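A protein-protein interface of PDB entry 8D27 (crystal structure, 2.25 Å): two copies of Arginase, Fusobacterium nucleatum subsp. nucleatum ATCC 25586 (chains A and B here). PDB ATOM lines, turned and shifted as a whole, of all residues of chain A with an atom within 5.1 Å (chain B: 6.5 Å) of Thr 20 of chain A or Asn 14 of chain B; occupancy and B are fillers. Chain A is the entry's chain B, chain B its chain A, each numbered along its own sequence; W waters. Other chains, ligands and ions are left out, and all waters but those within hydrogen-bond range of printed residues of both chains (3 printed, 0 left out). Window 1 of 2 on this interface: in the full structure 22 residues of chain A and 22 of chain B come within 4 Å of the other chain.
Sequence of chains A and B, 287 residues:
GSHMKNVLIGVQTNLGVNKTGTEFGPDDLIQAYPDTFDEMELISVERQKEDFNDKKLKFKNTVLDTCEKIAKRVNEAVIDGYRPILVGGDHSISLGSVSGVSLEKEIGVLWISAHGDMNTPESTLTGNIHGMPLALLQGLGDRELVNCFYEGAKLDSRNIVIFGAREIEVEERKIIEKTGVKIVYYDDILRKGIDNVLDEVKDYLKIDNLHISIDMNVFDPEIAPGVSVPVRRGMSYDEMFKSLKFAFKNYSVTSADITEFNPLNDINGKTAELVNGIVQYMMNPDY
OG1 of Thr 20 of chain B touches ND2 of Asn 14 of chain A (3.8 Å).
Asn 18 of chain B touches Thr 20 of chain A (C to OG1, 3.3 Å).
Thr 20 of chain B touches Thr 20 of chain A.
Thr 20 of chain A touches Phe 59 of chain B.
CE2 of Phe 59 of chain B touches CD1 of Leu 264 of chain A, at 3.7 Å.
The backbone carbonyl oxygen (O) of Lys 19 of chain B sits at hydrogen-bond distance from the side-chain amide nitrogen (ND2) of Asn 14 of chain B, 2.8 Å away.
OD1 of Asn 18 of chain B lies close to O of Leu 15 of chain B.
ND2 of Asn 18 of chain B is in hydrogen-bond range of O of Gly 16 of chain B (3.5 Å).
The backbone carbonyl oxygen (O) of Lys 19 of chain A is in hydrogen-bond range of the side-chain amide nitrogen (ND2) of Asn 14 of chain A (3.2 Å).
The side-chain amide nitrogen (ND2) of Asn 262 of chain A sits at hydrogen-bond distance from the backbone carbonyl oxygen (O) of Thr 20 of chain A (3.2 Å).
OD1 of Asn 262 of chain A lies close to N of Leu 264 of chain A (3.3 Å).
Of the printed residues of chain B, Thr 20 of chain A touches Asn 14, Asn 18, Lys 19, Thr 20 and Phe 59.
Of the printed residues of chain A, Asn 14 of chain B touches Thr 20.
Printed residues of chain B within 4 Å of Lys 19 of chain A: Thr 20 (3.3 Å).
Of the printed residues of chain B, Leu 264 of chain A touches Phe 59.
Of the printed residues of chain A, Asn 18 of chain B touches Thr 20 (3.3 Å).
Printed residues of chain A within 4 Å of Thr 20 of chain B: Asn 14, Asn 18, Lys 19 and Thr 20.
Of the printed residues of chain B, Asn 14 of chain A touches Thr 20 (3.8 Å).
The nearest printed residue of chain A that does not touch Asn 14 of chain B is Glu 23 of chain A (5.2 Å).
The nearest printed residue of chain A that does not touch Phe 59 of chain B is Gly 21 of chain A (4.8 Å).
The side-chain amide nitrogen of Asn 14 of chain B is in hydrogen-bond range of the side-chain hydroxyl of Thr 20 of chain A (3.3 Å).
N of Lys 19 of chain B is in hydrogen-bond range of OG1 of Thr 20 of chain A (3.4 Å).
The backbone carbonyl oxygen of Asn 18 of chain A sits close to the side-chain hydroxyl of Thr 20 of chain B (3.3 Å).
OG1 of Thr 20 of chain B is in hydrogen-bond range of N of Lys 19 of chain A (3.3 Å).
Hydrophobic or aromatic side chains of chain B that line the printed part of chain A: Phe 59.
Along chain B the printed residues that touch a printed residue of chain A span positions 14 to 59.
Among the printed residues, no Asp or Glu carboxylate lies within 4 Å of a Lys or Arg side-chain nitrogen of the other chain.
Water W3 lies within hydrogen-bond range of N of Thr 20 of chain A and O of Asn 18 of chain B.
Water W2 bridges the side-chain carboxylate of Glu 23 of chain B (3.0 Å) and the side-chain amide oxygen of Asn 14 of chain A (3.3 Å).
Water W1 lies within hydrogen-bond range of N of Thr 20 of chain B and O of Asn 18 of chain A.
Asn 14 of chain A touches Thr 20 of chain B, and with the chains exchanged Thr 20 of chain A touches Asn 14 of chain B.
Asn 18 of chain A touches Thr 20 of chain B, and with the chains exchanged Thr 20 of chain A touches Asn 18 of chain B.
Lys 19 of chain A touches Thr 20 of chain B, and with the chains exchanged Thr 20 of chain A touches Lys 19 of chain B.
Thr 20 of chain A touches its own counterpart, Thr 20 of chain B.
Positions printed for both chains: 14, 18, 19, 20, 21, 22 and 23.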
ATOM      1  N   ASN A  14      32.288 -31.303  21.868  1.00  0.00           N
ATOM      2  CA  ASN A  14      32.253 -29.851  21.747  1.00  0.00           C
ATOM      3  C   ASN A  14      32.531 -29.189  23.091  1.00  0.00           C
ATOM      4  O   ASN A  14      32.209 -28.007  23.269  1.00  0.00           O
ATOM      5  CB  ASN A  14      30.910 -29.377  21.196  1.00  0.00           C
ATOM      6  CG  ASN A  14      29.776 -29.579  22.174  1.00  0.00           C
ATOM      7  OD1 ASN A  14      29.790 -30.510  22.978  1.00  0.00           O
ATOM      8  ND2 ASN A  14      28.784 -28.706  22.109  1.00  0.00           N
ATOM      9  N   ASN A  18      32.159 -25.323  23.885  1.00  0.00           N
ATOM     10  CA  ASN A  18      31.000 -25.174  24.764  1.00  0.00           C
ATOM     11  C   ASN A  18      29.889 -24.385  24.075  1.00  0.00           C
ATOM     12  O   ASN A  18      29.219 -23.542  24.676  1.00  0.00           O
ATOM     13  CB  ASN A  18      31.405 -24.525  26.086  1.00  0.00           C
ATOM     14  CG  ASN A  18      32.331 -25.407  26.899  1.00  0.00           C
ATOM     15  OD1 ASN A  18      32.089 -26.604  27.046  1.00  0.00           O
ATOM     16  ND2 ASN A  18      33.402 -24.820  27.424  1.00  0.00           N
ATOM     17  N   LYS A  19      29.613 -24.701  22.815  1.00  0.00           N
ATOM     18  CA  LYS A  19      28.531 -24.109  22.015  1.00  0.00           C
ATOM     19  C   LYS A  19      28.058 -25.285  21.167  1.00  0.00           C
ATOM     20  O   LYS A  19      28.922 -25.911  20.564  1.00  0.00           O
ATOM     21  CB  LYS A  19      28.941 -22.859  21.239  1.00  0.00           C
ATOM     22  CG  LYS A  19      28.584 -21.515  21.843  1.00  0.00           C
ATOM     23  CD  LYS A  19      28.835 -20.384  20.878  1.00  0.00           C
ATOM     24  CE  LYS A  19      29.310 -19.116  21.544  1.00  0.00           C
ATOM     25  NZ  LYS A  19      29.510 -18.028  20.563  1.00  0.00           N
ATOM     26  N   THR A  20      26.770 -25.560  21.105  1.00  0.00           N
ATOM     27  CA  THR A  20      26.133 -26.699  20.408  1.00  0.00           C
ATOM     28  C   THR A  20      26.422 -26.745  18.911  1.00  0.00           C
ATOM     29  O   THR A  20      26.265 -25.702  18.307  1.00  0.00           O
ATOM     30  CB  THR A  20      24.613 -26.625  20.675  1.00  0.00           C
ATOM     31  OG1 THR A  20      24.466 -26.577  22.095  1.00  0.00           O
ATOM     32  CG2 THR A  20      23.839 -27.780  20.070  1.00  0.00           C
ATOM     33  N   GLY A  21      26.719 -27.922  18.367  1.00  0.00           N
ATOM     34  CA  GLY A  21      26.868 -28.136  16.920  1.00  0.00           C
ATOM     35  C   GLY A  21      28.070 -28.920  16.449  1.00  0.00           C
ATOM     36  O   GLY A  21      27.837 -29.929  15.831  1.00  0.00           O
ATOM     37  N   THR A  22      29.296 -28.531  16.790  1.00  0.00           N
ATOM     38  CA  THR A  22      30.543 -29.170  16.257  1.00  0.00           C
ATOM     39  C   THR A  22      30.698 -30.632  16.677  1.00  0.00           C
ATOM     40  O   THR A  22      31.328 -31.286  15.969  1.00  0.00           O
ATOM     41  CB  THR A  22      31.816 -28.333  16.481  1.00  0.00           C
ATOM     42  OG1 THR A  22      32.884 -28.772  15.644  1.00  0.00           O
ATOM     43  CG2 THR A  22      32.303 -28.363  17.912  1.00  0.00           C
ATOM     44  N   GLU A  23      30.100 -31.117  17.749  1.00  0.00           N
ATOM     45  CA  GLU A  23      30.098 -32.556  18.148  1.00  0.00           C
ATOM     46  C   GLU A  23      29.285 -33.389  17.150  1.00  0.00           C
ATOM     47  O   GLU A  23      29.404 -34.605  17.223  1.00  0.00           O
ATOM     48  CB  GLU A  23      29.595 -32.749  19.590  1.00  0.00           C
ATOM     49  CG  GLU A  23      28.069 -32.771  19.791  1.00  0.00           C
ATOM     50  CD  GLU A  23      27.319 -31.452  19.853  1.00  0.00           C
ATOM     51  OE1 GLU A  23      27.872 -30.426  19.464  1.00  0.00           O
ATOM     52  OE2 GLU A  23      26.169 -31.468  20.312  1.00  0.00           O
ATOM     53  N   ASN A 262      30.823 -26.789  12.525  1.00  0.00           N
ATOM     54  CA  ASN A 262      29.535 -26.742  13.197  1.00  0.00           C
ATOM     55  C   ASN A 262      28.438 -26.929  12.161  1.00  0.00           C
ATOM     56  O   ASN A 262      28.083 -25.969  11.462  1.00  0.00           O
ATOM     57  CB  ASN A 262      29.360 -25.413  13.932  1.00  0.00           C
ATOM     58  CG  ASN A 262      28.317 -25.487  15.019  1.00  0.00           C
ATOM     59  OD1 ASN A 262      27.140 -25.715  14.746  1.00  0.00           O
ATOM     60  ND2 ASN A 262      28.743 -25.307  16.262  1.00  0.00           N
ATOM     61  N   LEU A 264      25.285 -27.203  12.530  1.00  0.00           N
ATOM     62  CA  LEU A 264      24.026 -26.539  12.855  1.00  0.00           C
ATOM     63  C   LEU A 264      23.942 -25.163  12.209  1.00  0.00           C
ATOM     64  O   LEU A 264      22.870 -24.754  11.745  1.00  0.00           O
ATOM     65  CB  LEU A 264      23.873 -26.427  14.371  1.00  0.00           C
ATOM     66  CG  LEU A 264      22.545 -25.872  14.889  1.00  0.00           C
ATOM     67  CD1 LEU A 264      21.392 -26.791  14.529  1.00  0.00           C
ATOM     68  CD2 LEU A 264      22.608 -25.662  16.393  1.00  0.00           C
ATOM     69  N   ASN A 265      25.052 -24.432  12.178  1.00  0.00           N
ATOM     70  CA  ASN A 265      25.093 -23.106  11.582  1.00  0.00           C
ATOM     71  C   ASN A 265      25.459 -23.134  10.104  1.00  0.00           C
ATOM     72  O   ASN A 265      25.624 -22.070   9.500  1.00  0.00           O
ATOM     73  CB  ASN A 265      26.088 -22.219  12.336  1.00  0.00           C
ATOM     74  CG  ASN A 265      25.751 -22.085  13.807  1.00  0.00           C
ATOM     75  OD1 ASN A 265      25.181 -22.992  14.411  1.00  0.00           O
ATOM     76  ND2 ASN A 265      26.103 -20.947  14.392  1.00  0.00           N
ATOM     77  N   VAL B  11      18.092 -37.406  31.795  1.00  0.00           N
ATOM     78  CA  VAL B  11      18.220 -37.380  30.344  1.00  0.00           C
ATOM     79  C   VAL B  11      19.286 -36.350  30.008  1.00  0.00           C
ATOM     80  O   VAL B  11      19.046 -35.141  30.121  1.00  0.00           O
ATOM     81  CB  VAL B  11      16.894 -37.042  29.647  1.00  0.00           C
ATOM     82  CG1 VAL B  11      17.013 -37.282  28.150  1.00  0.00           C
ATOM     83  CG2 VAL B  11      15.751 -37.863  30.242  1.00  0.00           C
ATOM     84  N   GLN B  12      20.461 -36.821  29.592  1.00  0.00           N
ATOM     85  CA  GLN B  12      21.586 -35.935  29.301  1.00  0.00           C
ATOM     86  C   GLN B  12      21.469 -35.449  27.859  1.00  0.00           C
ATOM     87  O   GLN B  12      22.088 -35.979  26.934  1.00  0.00           O
ATOM     88  CB  GLN B  12      22.910 -36.650  29.541  1.00  0.00           C
ATOM     89  CG  GLN B  12      23.054 -37.274  30.916  1.00  0.00           C
ATOM     90  CD  GLN B  12      23.941 -38.504  30.901  1.00  0.00           C
ATOM     91  OE1 GLN B  12      23.646 -39.486  30.218  1.00  0.00           O
ATOM     92  NE2 GLN B  12      25.027 -38.464  31.666  1.00  0.00           N
ATOM     93  N   THR B  13      20.659 -34.408  27.671  1.00  0.00           N
ATOM     94  CA  THR B  13      20.509 -33.810  26.355  1.00  0.00           C
ATOM     95  C   THR B  13      20.294 -32.312  26.491  1.00  0.00           C
ATOM     96  O   THR B  13      19.847 -31.815  27.526  1.00  0.00           O
ATOM     97  CB  THR B  13      19.347 -34.432  25.570  1.00  0.00           C
ATOM     98  OG1 THR B  13      19.389 -33.980  24.211  1.00  0.00           O
ATOM     99  CG2 THR B  13      18.013 -34.043  26.189  1.00  0.00           C
ATOM    100  N   ASN B  14      20.636 -31.596  25.417  1.00  0.00           N
ATOM    101  CA  ASN B  14      20.371 -30.168  25.310  1.00  0.00           C
ATOM    102  C   ASN B  14      19.999 -29.796  23.879  1.00  0.00           C
ATOM    103  O   ASN B  14      20.031 -28.612  23.525  1.00  0.00           O
ATOM    104  CB  ASN B  14      21.580 -29.346  25.766  1.00  0.00           C
ATOM    105  CG  ASN B  14      22.799 -29.550  24.879  1.00  0.00           C
ATOM    106  OD1 ASN B  14      23.061 -30.655  24.405  1.00  0.00           O
ATOM    107  ND2 ASN B  14      23.553 -28.480  24.657  1.00  0.00           N
ATOM    108  N   LEU B  15      19.649 -30.780  23.052  1.00  0.00           N
ATOM    109  CA  LEU B  15      19.360 -30.550  21.643  1.00  0.00           C
ATOM    110  C   LEU B  15      18.005 -29.895  21.419  1.00  0.00           C
ATOM    111  O   LEU B  15      17.629 -29.660  20.264  1.00  0.00           O
ATOM    112  CB  LEU B  15      19.436 -31.872  20.879  1.00  0.00           C
ATOM    113  CG  LEU B  15      20.761 -32.621  21.038  1.00  0.00           C
ATOM    114  CD1 LEU B  15      20.759 -33.902  20.219  1.00  0.00           C
ATOM    115  CD2 LEU B  15      21.936 -31.735  20.650  1.00  0.00           C
ATOM    116  N   GLY B  16      17.266 -29.607  22.485  1.00  0.00           N
ATOM    117  CA  GLY B  16      16.082 -28.786  22.376  1.00  0.00           C
ATOM    118  C   GLY B  16      16.423 -27.327  22.587  1.00  0.00           C
ATOM    119  O   GLY B  16      15.986 -26.465  21.823  1.00  0.00           O
ATOM    120  N   VAL B  17      17.218 -27.043  23.620  1.00  0.00           N
ATOM    121  CA  VAL B  17      17.597 -25.664  23.904  1.00  0.00           C
ATOM    122  C   VAL B  17      18.781 -25.236  23.047  1.00  0.00           C
ATOM    123  O   VAL B  17      18.942 -24.044  22.756  1.00  0.00           O
ATOM    124  CB  VAL B  17      17.903 -25.493  25.403  1.00  0.00           C
ATOM    125  CG1 VAL B  17      19.108 -26.331  25.812  1.00  0.00           C
ATOM    126  CG2 VAL B  17      18.136 -24.025  25.731  1.00  0.00           C
ATOM    127  N   ASN B  18      19.620 -26.183  22.629  1.00  0.00           N
ATOM    128  CA  ASN B  18      20.773 -25.889  21.780  1.00  0.00           C
ATOM    129  C   ASN B  18      21.666 -24.830  22.427  1.00  0.00           C
ATOM    130  O   ASN B  18      22.074 -23.851  21.802  1.00  0.00           O
ATOM    131  CB  ASN B  18      20.320 -25.457  20.384  1.00  0.00           C
ATOM    132  CG  ASN B  18      19.392 -26.468  19.734  1.00  0.00           C
ATOM    133  OD1 ASN B  18      19.684 -27.662  19.702  1.00  0.00           O
ATOM    134  ND2 ASN B  18      18.267 -25.992  19.215  1.00  0.00           N
ATOM    135  N   LYS B  19      21.952 -25.032  23.709  1.00  0.00           N
ATOM    136  CA  LYS B  19      22.937 -24.255  24.443  1.00  0.00           C
ATOM    137  C   LYS B  19      23.572 -25.237  25.419  1.00  0.00           C
ATOM    138  O   LYS B  19      22.867 -26.080  25.985  1.00  0.00           O
ATOM    139  CB  LYS B  19      22.314 -23.069  25.182  1.00  0.00           C
ATOM    140  CG  LYS B  19      23.320 -22.195  25.927  1.00  0.00           C
ATOM    141  CD  LYS B  19      22.923 -22.005  27.387  1.00  0.00           C
ATOM    142  CE  LYS B  19      23.942 -21.165  28.146  1.00  0.00           C
ATOM    143  NZ  LYS B  19      24.926 -21.992  28.904  1.00  0.00           N
ATOM    144  N   THR B  20      24.885 -25.131  25.608  1.00  0.00           N
ATOM    145  CA  THR B  20      25.634 -26.148  26.338  1.00  0.00           C
ATOM    146  C   THR B  20      25.476 -25.987  27.847  1.00  0.00           C
ATOM    147  O   THR B  20      25.665 -24.893  28.388  1.00  0.00           O
ATOM    148  CB  THR B  20      27.117 -26.076  25.961  1.00  0.00           C
ATOM    149  OG1 THR B  20      27.270 -26.256  24.546  1.00  0.00           O
ATOM    150  CG2 THR B  20      27.911 -27.147  26.681  1.00  0.00           C
ATOM    151  N   GLY B  21      25.146 -27.086  28.526  1.00  0.00           N
ATOM    152  CA  GLY B  21      25.051 -27.084  29.971  1.00  0.00           C
ATOM    153  C   GLY B  21      24.070 -28.092  30.535  1.00  0.00           C
ATOM    154  O   GLY B  21      24.442 -28.935  31.356  1.00  0.00           O
ATOM    155  N   THR B  22      22.809 -28.020  30.097  1.00  0.00           N
ATOM    156  CA  THR B  22      21.767 -28.838  30.711  1.00  0.00           C
ATOM    157  C   THR B  22      21.987 -30.330  30.494  1.00  0.00           C
ATOM    158  O   THR B  22      21.487 -31.135  31.288  1.00  0.00           O
ATOM    159  CB  THR B  22      20.385 -28.447  30.174  1.00  0.00           C
ATOM    160  OG1 THR B  22      20.345 -28.619  28.751  1.00  0.00           O
ATOM    161  CG2 THR B  22      20.066 -27.001  30.527  1.00  0.00           C
ATOM    162  N   GLU B  23      22.706 -30.721  29.439  1.00  0.00           N
ATOM    163  CA  GLU B  23      22.984 -32.139  29.239  1.00  0.00           C
ATOM    164  C   GLU B  23      23.863 -32.699  30.349  1.00  0.00           C
ATOM    165  O   GLU B  23      23.875 -33.915  30.562  1.00  0.00           O
ATOM    166  CB  GLU B  23      23.627 -32.368  27.868  1.00  0.00           C
ATOM    167  CG  GLU B  23      25.070 -31.900  27.730  1.00  0.00           C
ATOM    168  CD  GLU B  23      25.185 -30.421  27.408  1.00  0.00           C
ATOM    169  OE1 GLU B  23      24.327 -29.638  27.862  1.00  0.00           O
ATOM    170  OE2 GLU B  23      26.135 -30.037  26.696  1.00  0.00           O
ATOM    171  N   VAL B  45      22.133 -39.563  24.415  1.00  0.00           N
ATOM    172  CA  VAL B  45      21.728 -39.129  23.083  1.00  0.00           C
ATOM    173  C   VAL B  45      22.314 -40.087  22.054  1.00  0.00           C
ATOM    174  O   VAL B  45      23.537 -40.223  21.945  1.00  0.00           O
ATOM    175  CB  VAL B  45      22.177 -37.687  22.809  1.00  0.00           C
ATOM    176  CG1 VAL B  45      22.108 -37.382  21.318  1.00  0.00           C
ATOM    177  CG2 VAL B  45      21.328 -36.706  23.608  1.00  0.00           C
ATOM    178  N   PHE B  59      17.553 -30.438  15.161  1.00  0.00           N
ATOM    179  CA  PHE B  59      17.738 -31.760  15.752  1.00  0.00           C
ATOM    180  C   PHE B  59      16.392 -32.453  15.945  1.00  0.00           C
ATOM    181  O   PHE B  59      16.066 -32.942  17.028  1.00  0.00           O
ATOM    182  CB  PHE B  59      18.503 -31.670  17.074  1.00  0.00           C
ATOM    183  CG  PHE B  59      19.855 -31.029  16.948  1.00  0.00           C
ATOM    184  CD1 PHE B  59      20.906 -31.705  16.353  1.00  0.00           C
ATOM    185  CD2 PHE B  59      20.075 -29.749  17.426  1.00  0.00           C
ATOM    186  CE1 PHE B  59      22.153 -31.115  16.237  1.00  0.00           C
ATOM    187  CE2 PHE B  59      21.317 -29.155  17.314  1.00  0.00           C
ATOM    188  CZ  PHE B  59      22.358 -29.839  16.718  1.00  0.00           C
ATOM    189  N   VAL B  63      16.241 -35.436  18.805  1.00  0.00           N
ATOM    190  CA  VAL B  63      15.360 -35.143  19.930  1.00  0.00           C
ATOM    191  C   VAL B  63      14.188 -36.114  19.949  1.00  0.00           C
ATOM    192  O   VAL B  63      13.722 -36.535  21.014  1.00  0.00           O
ATOM    193  CB  VAL B  63      14.885 -33.680  19.855  1.00  0.00           C
ATOM    194  CG1 VAL B  63      13.771 -33.425  20.858  1.00  0.00           C
ATOM    195  CG2 VAL B  63      16.053 -32.730  20.084  1.00  0.00           C
ATOM    196  N   GLY B  89      18.752 -31.464  31.738  1.00  0.00           N
ATOM    197  CA  GLY B  89      18.106 -31.716  30.461  1.00  0.00           C
ATOM    198  C   GLY B  89      17.075 -30.654  30.121  1.00  0.00           C
ATOM    199  O   GLY B  89      16.326 -30.221  30.993  1.00  0.00           O
ATOM    200  N   ASP B  90      17.032 -30.237  28.857  1.00  0.00           N
ATOM    201  CA  ASP B  90      16.123 -29.178  28.441  1.00  0.00           C
ATOM    202  C   ASP B  90      14.680 -29.685  28.469  1.00  0.00           C
ATOM    203  O   ASP B  90      14.401 -30.846  28.780  1.00  0.00           O
ATOM    204  CB  ASP B  90      16.511 -28.657  27.057  1.00  0.00           C
ATOM    205  CG  ASP B  90      16.197 -29.640  25.951  1.00  0.00           C
ATOM    206  OD1 ASP B  90      17.017 -30.545  25.700  1.00  0.00           O
ATOM    207  OD2 ASP B  90      15.125 -29.509  25.328  1.00  0.00           O
ATOM    208  N   SER B  92      12.376 -30.233  26.198  1.00  0.00           N
ATOM    209  CA  SER B  92      11.821 -31.134  25.197  1.00  0.00           C
ATOM    210  C   SER B  92      11.618 -32.542  25.742  1.00  0.00           C
ATOM    211  O   SER B  92      10.766 -33.276  25.228  1.00  0.00           O
ATOM    212  CB  SER B  92      12.724 -31.176  23.963  1.00  0.00           C
ATOM    213  OG  SER B  92      14.058 -31.499  24.310  1.00  0.00           O
HETATM  214  O   HOH W   1      25.978 -22.645  24.139  1.00  0.00           O
HETATM  215  O   HOH W   2      27.753 -32.008  25.058  1.00  0.00           O
HETATM  216  O   HOH W   3      25.380 -23.139  21.402  1.00  0.00           O
